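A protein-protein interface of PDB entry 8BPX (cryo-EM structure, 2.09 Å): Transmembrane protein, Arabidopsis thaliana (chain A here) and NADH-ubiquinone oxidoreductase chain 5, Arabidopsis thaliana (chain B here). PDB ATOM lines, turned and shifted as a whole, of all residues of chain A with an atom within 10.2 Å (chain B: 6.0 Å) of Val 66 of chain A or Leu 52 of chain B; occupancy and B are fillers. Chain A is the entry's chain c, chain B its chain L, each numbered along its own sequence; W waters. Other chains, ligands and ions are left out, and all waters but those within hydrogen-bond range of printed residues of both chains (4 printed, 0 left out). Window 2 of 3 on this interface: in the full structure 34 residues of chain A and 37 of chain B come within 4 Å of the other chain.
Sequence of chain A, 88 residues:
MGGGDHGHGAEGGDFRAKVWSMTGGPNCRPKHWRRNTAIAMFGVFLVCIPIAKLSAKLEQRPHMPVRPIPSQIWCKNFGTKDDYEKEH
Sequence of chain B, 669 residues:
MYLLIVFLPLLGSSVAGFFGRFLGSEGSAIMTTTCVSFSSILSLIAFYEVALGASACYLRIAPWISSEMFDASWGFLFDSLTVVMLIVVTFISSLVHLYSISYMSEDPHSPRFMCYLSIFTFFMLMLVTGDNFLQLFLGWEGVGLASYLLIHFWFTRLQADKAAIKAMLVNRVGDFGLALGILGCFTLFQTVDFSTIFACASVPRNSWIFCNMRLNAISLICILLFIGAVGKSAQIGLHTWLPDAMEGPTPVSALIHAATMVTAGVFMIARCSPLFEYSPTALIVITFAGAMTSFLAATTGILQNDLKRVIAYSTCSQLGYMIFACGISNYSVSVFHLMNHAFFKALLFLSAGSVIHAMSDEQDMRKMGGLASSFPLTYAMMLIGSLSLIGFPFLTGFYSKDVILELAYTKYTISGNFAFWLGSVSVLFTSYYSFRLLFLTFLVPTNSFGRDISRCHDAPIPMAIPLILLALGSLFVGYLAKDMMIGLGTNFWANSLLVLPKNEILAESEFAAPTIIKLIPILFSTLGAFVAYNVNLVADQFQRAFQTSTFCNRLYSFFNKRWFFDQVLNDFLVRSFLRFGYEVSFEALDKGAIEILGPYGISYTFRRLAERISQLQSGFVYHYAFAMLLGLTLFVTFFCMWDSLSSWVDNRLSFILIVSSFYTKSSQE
Water W3 bridges OH of Tyr 48 of chain B (2.6 Å) and O of Pro 68 of chain A (2.8 Å). Water W2 bridges the backbone NH (N) of His 63 of chain A and the side-chain hydroxyl (OG) of Ser 55 of chain B. Water W4 lies within hydrogen-bond range of O of Tyr 48 of chain B (2.8 Å), NH1 of Arg 67 of chain A (3.1 Å) and N of Gly 53 of chain B (3.4 Å). Water W1 bridges the backbone carbonyl oxygen (O) of Leu 52 of chain B (2.8 Å) and the guanidinium group (NH1) of Arg 67 of chain A (2.9 Å).
The side-chain carboxylate of Glu 49 of chain B lies within salt-bridge range of the guanidinium group of Arg 61 of chain A (3.2 Å). The backbone NH (N) of Val 66 of chain A sits at hydrogen-bond distance from the backbone carbonyl oxygen (O) of Gly 53 of chain B (3.2 Å). O of Ser 55 of chain B sits at hydrogen-bond distance from NH2 of Arg 61 of chain A (3.0 Å). The side-chain hydroxyl (OG) of Ser 55 of chain B sits at hydrogen-bond distance from the backbone carbonyl oxygen (O) of His 63 of chain A (2.7 Å).
Val 66 of chain A touches just these residues of chain B: Leu 52 and Gly 53. Pro 68 of chain A touches none of the printed residues of chain B. Of the printed residues of chain B, Ile 69 of chain A touches Glu 49. Printed residues of chain A within 4 Å of Glu 49 of chain B: Arg 61 and Ile 69. No residue of chain A comes within 4 Å of Ala 51 of chain B. Leu 52 of chain B touches just these residues of chain A: Val 66 (3.7 Å) and Arg 67 (3.5 Å). Gly 53 of chain B touches two residues of chain A. The nearest printed residue of chain B that does not touch Pro 65 of chain A is Ser 55 of chain B (4.05 Å).
Printed residues of chain A that touch a printed residue of chain B: Arg 61, His 63, Pro 65, Val 66, Arg 67 and Ile 69.
Among the printed residues, pairs that only touch across the chains: His 63 of chain A with Ala 54 of chain B, Pro 65 of chain A with Gly 53 of chain B, Val 66 of chain A with Leu 52 of chain B, Arg 67 of chain A with Tyr 48 of chain B, Arg 67 of chain A with Leu 52 of chain B and Ile 69 of chain A with Glu 49 of chain B.
The backbone carbonyl oxygen of Phe 47 of chain B sits at hydrogen-bond distance from the backbone NH of Leu 52 of chain B (3.3 Å). O of Tyr 48 of chain B sits at hydrogen-bond distance from N of Gly 53 of chain B (3.0 Å). O of Val 50 of chain B is in hydrogen-bond range of N of Ser 55 of chain B, at 3.2 Å. The backbone NH (N) of Ile 69 of chain A is in hydrogen-bond range of the side-chain amide oxygen (OE1) of Gln 72 of chain A (3.1 Å).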
ATOM      1  N   ARG A  61      -1.526 -24.106   1.715  1.00  0.00           N
ATOM      2  CA  ARG A  61      -0.270 -23.397   1.963  1.00  0.00           C
ATOM      3  C   ARG A  61      -0.539 -21.899   1.922  1.00  0.00           C
ATOM      4  O   ARG A  61      -0.491 -21.279   0.850  1.00  0.00           O
ATOM      5  CB  ARG A  61       0.796 -23.796   0.946  1.00  0.00           C
ATOM      6  CG  ARG A  61       0.807 -25.272   0.575  1.00  0.00           C
ATOM      7  CD  ARG A  61       1.133 -26.153   1.775  1.00  0.00           C
ATOM      8  NE  ARG A  61       2.517 -26.011   2.206  1.00  0.00           N
ATOM      9  CZ  ARG A  61       3.553 -26.603   1.628  1.00  0.00           C
ATOM     10  NH1 ARG A  61       3.401 -27.400   0.587  1.00  0.00           N
ATOM     11  NH2 ARG A  61       4.773 -26.384   2.108  1.00  0.00           N
ATOM     12  N   HIS A  63       1.238 -19.425   2.747  1.00  0.00           N
ATOM     13  CA  HIS A  63       2.411 -18.594   2.519  1.00  0.00           C
ATOM     14  C   HIS A  63       3.199 -19.105   1.328  1.00  0.00           C
ATOM     15  O   HIS A  63       3.495 -20.301   1.239  1.00  0.00           O
ATOM     16  CB  HIS A  63       3.305 -18.558   3.755  1.00  0.00           C
ATOM     17  CG  HIS A  63       2.735 -17.752   4.873  1.00  0.00           C
ATOM     18  ND1 HIS A  63       2.021 -16.594   4.658  1.00  0.00           N
ATOM     19  CD2 HIS A  63       2.750 -17.943   6.212  1.00  0.00           C
ATOM     20  CE1 HIS A  63       1.631 -16.102   5.818  1.00  0.00           C
ATOM     21  NE2 HIS A  63       2.060 -16.902   6.777  1.00  0.00           N
ATOM     22  N   MET A  64       3.537 -18.199   0.425  1.00  0.00           N
ATOM     23  CA  MET A  64       4.452 -18.529  -0.652  1.00  0.00           C
ATOM     24  C   MET A  64       5.813 -18.881  -0.065  1.00  0.00           C
ATOM     25  O   MET A  64       6.294 -18.177   0.832  1.00  0.00           O
ATOM     26  CB  MET A  64       4.584 -17.357  -1.619  1.00  0.00           C
ATOM     27  CG  MET A  64       3.333 -17.062  -2.401  1.00  0.00           C
ATOM     28  SD  MET A  64       2.602 -18.523  -3.160  1.00  0.00           S
ATOM     29  CE  MET A  64       3.687 -18.725  -4.561  1.00  0.00           C
ATOM     30  N   PRO A  65       6.447 -19.956  -0.517  1.00  0.00           N
ATOM     31  CA  PRO A  65       7.774 -20.299  -0.002  1.00  0.00           C
ATOM     32  C   PRO A  65       8.829 -19.322  -0.499  1.00  0.00           C
ATOM     33  O   PRO A  65       8.653 -18.626  -1.500  1.00  0.00           O
ATOM     34  CB  PRO A  65       8.011 -21.708  -0.551  1.00  0.00           C
ATOM     35  CG  PRO A  65       7.208 -21.745  -1.800  1.00  0.00           C
ATOM     36  CD  PRO A  65       5.980 -20.924  -1.524  1.00  0.00           C
ATOM     37  N   VAL A  66       9.941 -19.277   0.235  1.00  0.00           N
ATOM     38  CA  VAL A  66      11.002 -18.329  -0.089  1.00  0.00           C
ATOM     39  C   VAL A  66      11.671 -18.699  -1.408  1.00  0.00           C
ATOM     40  O   VAL A  66      12.063 -17.825  -2.186  1.00  0.00           O
ATOM     41  CB  VAL A  66      12.014 -18.247   1.068  1.00  0.00           C
ATOM     42  CG1 VAL A  66      11.382 -17.563   2.259  1.00  0.00           C
ATOM     43  CG2 VAL A  66      12.525 -19.625   1.450  1.00  0.00           C
ATOM     44  N   ARG A  67      11.818 -19.987  -1.673  1.00  0.00           N
ATOM     45  CA  ARG A  67      12.337 -20.516  -2.921  1.00  0.00           C
ATOM     46  C   ARG A  67      11.343 -21.541  -3.442  1.00  0.00           C
ATOM     47  O   ARG A  67      10.483 -22.012  -2.690  1.00  0.00           O
ATOM     48  CB  ARG A  67      13.721 -21.160  -2.738  1.00  0.00           C
ATOM     49  CG  ARG A  67      13.834 -22.100  -1.567  1.00  0.00           C
ATOM     50  CD  ARG A  67      15.237 -22.663  -1.462  1.00  0.00           C
ATOM     51  NE  ARG A  67      16.155 -21.743  -0.803  1.00  0.00           N
ATOM     52  CZ  ARG A  67      16.179 -21.513   0.500  1.00  0.00           C
ATOM     53  NH1 ARG A  67      15.341 -22.119   1.324  1.00  0.00           N
ATOM     54  NH2 ARG A  67      17.067 -20.655   0.991  1.00  0.00           N
ATOM     55  N   PRO A  68      11.402 -21.876  -4.730  1.00  0.00           N
ATOM     56  CA  PRO A  68      10.460 -22.864  -5.276  1.00  0.00           C
ATOM     57  C   PRO A  68      10.596 -24.219  -4.593  1.00  0.00           C
ATOM     58  O   PRO A  68      11.697 -24.656  -4.254  1.00  0.00           O
ATOM     59  CB  PRO A  68      10.848 -22.936  -6.757  1.00  0.00           C
ATOM     60  CG  PRO A  68      12.236 -22.400  -6.815  1.00  0.00           C
ATOM     61  CD  PRO A  68      12.277 -21.331  -5.782  1.00  0.00           C
ATOM     62  N   ILE A  69       9.464 -24.888  -4.405  1.00  0.00           N
ATOM     63  CA  ILE A  69       9.435 -26.150  -3.669  1.00  0.00           C
ATOM     64  C   ILE A  69       8.710 -27.197  -4.505  1.00  0.00           C
ATOM     65  O   ILE A  69       7.912 -26.860  -5.393  1.00  0.00           O
ATOM     66  CB  ILE A  69       8.769 -25.991  -2.282  1.00  0.00           C
ATOM     67  CG1 ILE A  69       7.377 -25.370  -2.404  1.00  0.00           C
ATOM     68  CG2 ILE A  69       9.660 -25.200  -1.347  1.00  0.00           C
ATOM     69  CD1 ILE A  69       6.575 -25.439  -1.131  1.00  0.00           C
ATOM     70  N   GLN A  72       4.801 -27.225  -5.231  1.00  0.00           N
ATOM     71  CA  GLN A  72       4.248 -26.287  -6.202  1.00  0.00           C
ATOM     72  C   GLN A  72       3.941 -26.939  -7.541  1.00  0.00           C
ATOM     73  O   GLN A  72       3.182 -26.372  -8.330  1.00  0.00           O
ATOM     74  CB  GLN A  72       5.215 -25.124  -6.395  1.00  0.00           C
ATOM     75  CG  GLN A  72       5.103 -24.059  -5.329  1.00  0.00           C
ATOM     76  CD  GLN A  72       6.191 -23.019  -5.443  1.00  0.00           C
ATOM     77  OE1 GLN A  72       7.278 -23.304  -5.933  1.00  0.00           O
ATOM     78  NE2 GLN A  72       5.899 -21.804  -5.004  1.00  0.00           N
ATOM     79  N   PHE A  78      -1.672 -22.355  -2.952  1.00  0.00           N
ATOM     80  CA  PHE A  78      -0.686 -21.429  -2.415  1.00  0.00           C
ATOM     81  C   PHE A  78      -1.251 -20.015  -2.420  1.00  0.00           C
ATOM     82  O   PHE A  78      -1.701 -19.526  -3.462  1.00  0.00           O
ATOM     83  CB  PHE A  78       0.619 -21.487  -3.215  1.00  0.00           C
ATOM     84  CG  PHE A  78       1.477 -22.673  -2.886  1.00  0.00           C
ATOM     85  CD1 PHE A  78       1.252 -23.900  -3.489  1.00  0.00           C
ATOM     86  CD2 PHE A  78       2.493 -22.569  -1.955  1.00  0.00           C
ATOM     87  CE1 PHE A  78       2.032 -24.993  -3.176  1.00  0.00           C
ATOM     88  CE2 PHE A  78       3.275 -23.658  -1.638  1.00  0.00           C
ATOM     89  CZ  PHE A  78       3.046 -24.871  -2.250  1.00  0.00           C
ATOM     90  N   PHE B  47      10.710 -31.054   5.560  1.00  0.00           N
ATOM     91  CA  PHE B  47      11.537 -30.142   6.341  1.00  0.00           C
ATOM     92  C   PHE B  47      12.096 -29.039   5.455  1.00  0.00           C
ATOM     93  O   PHE B  47      12.143 -27.872   5.857  1.00  0.00           O
ATOM     94  CB  PHE B  47      12.676 -30.898   7.022  1.00  0.00           C
ATOM     95  CG  PHE B  47      13.577 -30.022   7.852  1.00  0.00           C
ATOM     96  CD1 PHE B  47      14.698 -29.428   7.296  1.00  0.00           C
ATOM     97  CD2 PHE B  47      13.304 -29.801   9.189  1.00  0.00           C
ATOM     98  CE1 PHE B  47      15.521 -28.617   8.054  1.00  0.00           C
ATOM     99  CE2 PHE B  47      14.128 -28.998   9.957  1.00  0.00           C
ATOM    100  CZ  PHE B  47      15.240 -28.406   9.388  1.00  0.00           C
ATOM    101  N   TYR B  48      12.525 -29.399   4.248  1.00  0.00           N
ATOM    102  CA  TYR B  48      13.008 -28.397   3.306  1.00  0.00           C
ATOM    103  C   TYR B  48      11.899 -27.416   2.936  1.00  0.00           C
ATOM    104  O   TYR B  48      12.131 -26.207   2.845  1.00  0.00           O
ATOM    105  CB  TYR B  48      13.570 -29.093   2.068  1.00  0.00           C
ATOM    106  CG  TYR B  48      14.079 -28.188   0.969  1.00  0.00           C
ATOM    107  CD1 TYR B  48      13.246 -27.765  -0.054  1.00  0.00           C
ATOM    108  CD2 TYR B  48      15.408 -27.788   0.941  1.00  0.00           C
ATOM    109  CE1 TYR B  48      13.721 -26.951  -1.067  1.00  0.00           C
ATOM    110  CE2 TYR B  48      15.887 -26.977  -0.060  1.00  0.00           C
ATOM    111  CZ  TYR B  48      15.042 -26.561  -1.061  1.00  0.00           C
ATOM    112  OH  TYR B  48      15.526 -25.755  -2.059  1.00  0.00           O
ATOM    113  N   GLU B  49      10.682 -27.924   2.738  1.00  0.00           N
ATOM    114  CA  GLU B  49       9.567 -27.099   2.280  1.00  0.00           C
ATOM    115  C   GLU B  49       9.015 -26.188   3.376  1.00  0.00           C
ATOM    116  O   GLU B  49       8.710 -25.019   3.118  1.00  0.00           O
ATOM    117  CB  GLU B  49       8.452 -27.998   1.744  1.00  0.00           C
ATOM    118  CG  GLU B  49       8.545 -28.294   0.273  1.00  0.00           C
ATOM    119  CD  GLU B  49       7.303 -28.963  -0.271  1.00  0.00           C
ATOM    120  OE1 GLU B  49       6.220 -28.788   0.321  1.00  0.00           O
ATOM    121  OE2 GLU B  49       7.407 -29.652  -1.303  1.00  0.00           O
ATOM    122  N   VAL B  50       8.870 -26.701   4.591  1.00  0.00           N
ATOM    123  CA  VAL B  50       8.117 -26.037   5.651  1.00  0.00           C
ATOM    124  C   VAL B  50       9.013 -25.180   6.529  1.00  0.00           C
ATOM    125  O   VAL B  50       8.703 -24.020   6.798  1.00  0.00           O
ATOM    126  CB  VAL B  50       7.346 -27.080   6.495  1.00  0.00           C
ATOM    127  CG1 VAL B  50       6.770 -26.442   7.751  1.00  0.00           C
ATOM    128  CG2 VAL B  50       6.253 -27.740   5.670  1.00  0.00           C
ATOM    129  N   ALA B  51      10.117 -25.744   7.008  1.00  0.00           N
ATOM    130  CA  ALA B  51      10.988 -25.015   7.920  1.00  0.00           C
ATOM    131  C   ALA B  51      11.954 -24.112   7.160  1.00  0.00           C
ATOM    132  O   ALA B  51      12.015 -22.905   7.407  1.00  0.00           O
ATOM    133  CB  ALA B  51      11.746 -25.998   8.816  1.00  0.00           C
ATOM    134  N   LEU B  52      12.719 -24.683   6.228  1.00  0.00           N
ATOM    135  CA  LEU B  52      13.662 -23.880   5.454  1.00  0.00           C
ATOM    136  C   LEU B  52      12.937 -22.963   4.476  1.00  0.00           C
ATOM    137  O   LEU B  52      13.380 -21.835   4.232  1.00  0.00           O
ATOM    138  CB  LEU B  52      14.645 -24.789   4.719  1.00  0.00           C
ATOM    139  CG  LEU B  52      15.396 -25.797   5.592  1.00  0.00           C
ATOM    140  CD1 LEU B  52      16.330 -26.647   4.759  1.00  0.00           C
ATOM    141  CD2 LEU B  52      16.154 -25.102   6.708  1.00  0.00           C
ATOM    142  N   GLY B  53      11.827 -23.427   3.908  1.00  0.00           N
ATOM    143  CA  GLY B  53      11.040 -22.624   2.991  1.00  0.00           C
ATOM    144  C   GLY B  53      10.047 -21.683   3.635  1.00  0.00           C
ATOM    145  O   GLY B  53       9.469 -20.851   2.932  1.00  0.00           O
ATOM    146  N   ALA B  54       9.838 -21.799   4.947  1.00  0.00           N
ATOM    147  CA  ALA B  54       8.897 -20.960   5.691  1.00  0.00           C
ATOM    148  C   ALA B  54       7.500 -21.006   5.073  1.00  0.00           C
ATOM    149  O   ALA B  54       6.863 -19.981   4.833  1.00  0.00           O
ATOM    150  CB  ALA B  54       9.407 -19.519   5.796  1.00  0.00           C
ATOM    151  N   SER B  55       7.021 -22.223   4.813  1.00  0.00           N
ATOM    152  CA  SER B  55       5.707 -22.441   4.200  1.00  0.00           C
ATOM    153  C   SER B  55       5.018 -23.589   4.937  1.00  0.00           C
ATOM    154  O   SER B  55       5.163 -24.757   4.570  1.00  0.00           O
ATOM    155  CB  SER B  55       5.840 -22.723   2.711  1.00  0.00           C
ATOM    156  OG  SER B  55       4.592 -22.611   2.057  1.00  0.00           O
ATOM    157  N   MET B 484      20.348 -22.063  13.497  1.00  0.00           N
ATOM    158  CA  MET B 484      18.945 -22.284  13.042  1.00  0.00           C
ATOM    159  C   MET B 484      17.952 -22.361  14.193  1.00  0.00           C
ATOM    160  O   MET B 484      17.015 -21.692  14.141  1.00  0.00           O
ATOM    161  CB  MET B 484      18.832 -23.580  12.238  1.00  0.00           C
ATOM    162  CG  MET B 484      17.609 -23.760  11.426  1.00  0.00           C
ATOM    163  SD  MET B 484      17.724 -25.304  10.500  1.00  0.00           S
ATOM    164  CE  MET B 484      18.095 -26.451  11.820  1.00  0.00           C
ATOM    165  N   PHE B 492      13.518 -19.172  12.613  1.00  0.00           N
ATOM    166  CA  PHE B 492      13.340 -20.514  12.064  1.00  0.00           C
ATOM    167  C   PHE B 492      12.025 -21.137  12.528  1.00  0.00           C
ATOM    168  O   PHE B 492      11.362 -21.840  11.761  1.00  0.00           O
ATOM    169  CB  PHE B 492      14.537 -21.382  12.459  1.00  0.00           C
ATOM    170  CG  PHE B 492      14.287 -22.861  12.368  1.00  0.00           C
ATOM    171  CD1 PHE B 492      14.389 -23.517  11.150  1.00  0.00           C
ATOM    172  CD2 PHE B 492      13.975 -23.600  13.500  1.00  0.00           C
ATOM    173  CE1 PHE B 492      14.175 -24.876  11.060  1.00  0.00           C
ATOM    174  CE2 PHE B 492      13.751 -24.963  13.416  1.00  0.00           C
ATOM    175  CZ  PHE B 492      13.854 -25.603  12.194  1.00  0.00           C
HETATM  176  O   HOH W   1      16.143 -21.757   4.104  1.00  0.00           O
HETATM  177  O   HOH W   2       2.203 -21.683   3.918  1.00  0.00           O
HETATM  178  O   HOH W   3      14.469 -24.672  -4.156  1.00  0.00           O
HETATM  179  O   HOH W   4      13.347 -24.535   1.020  1.00  0.00           O
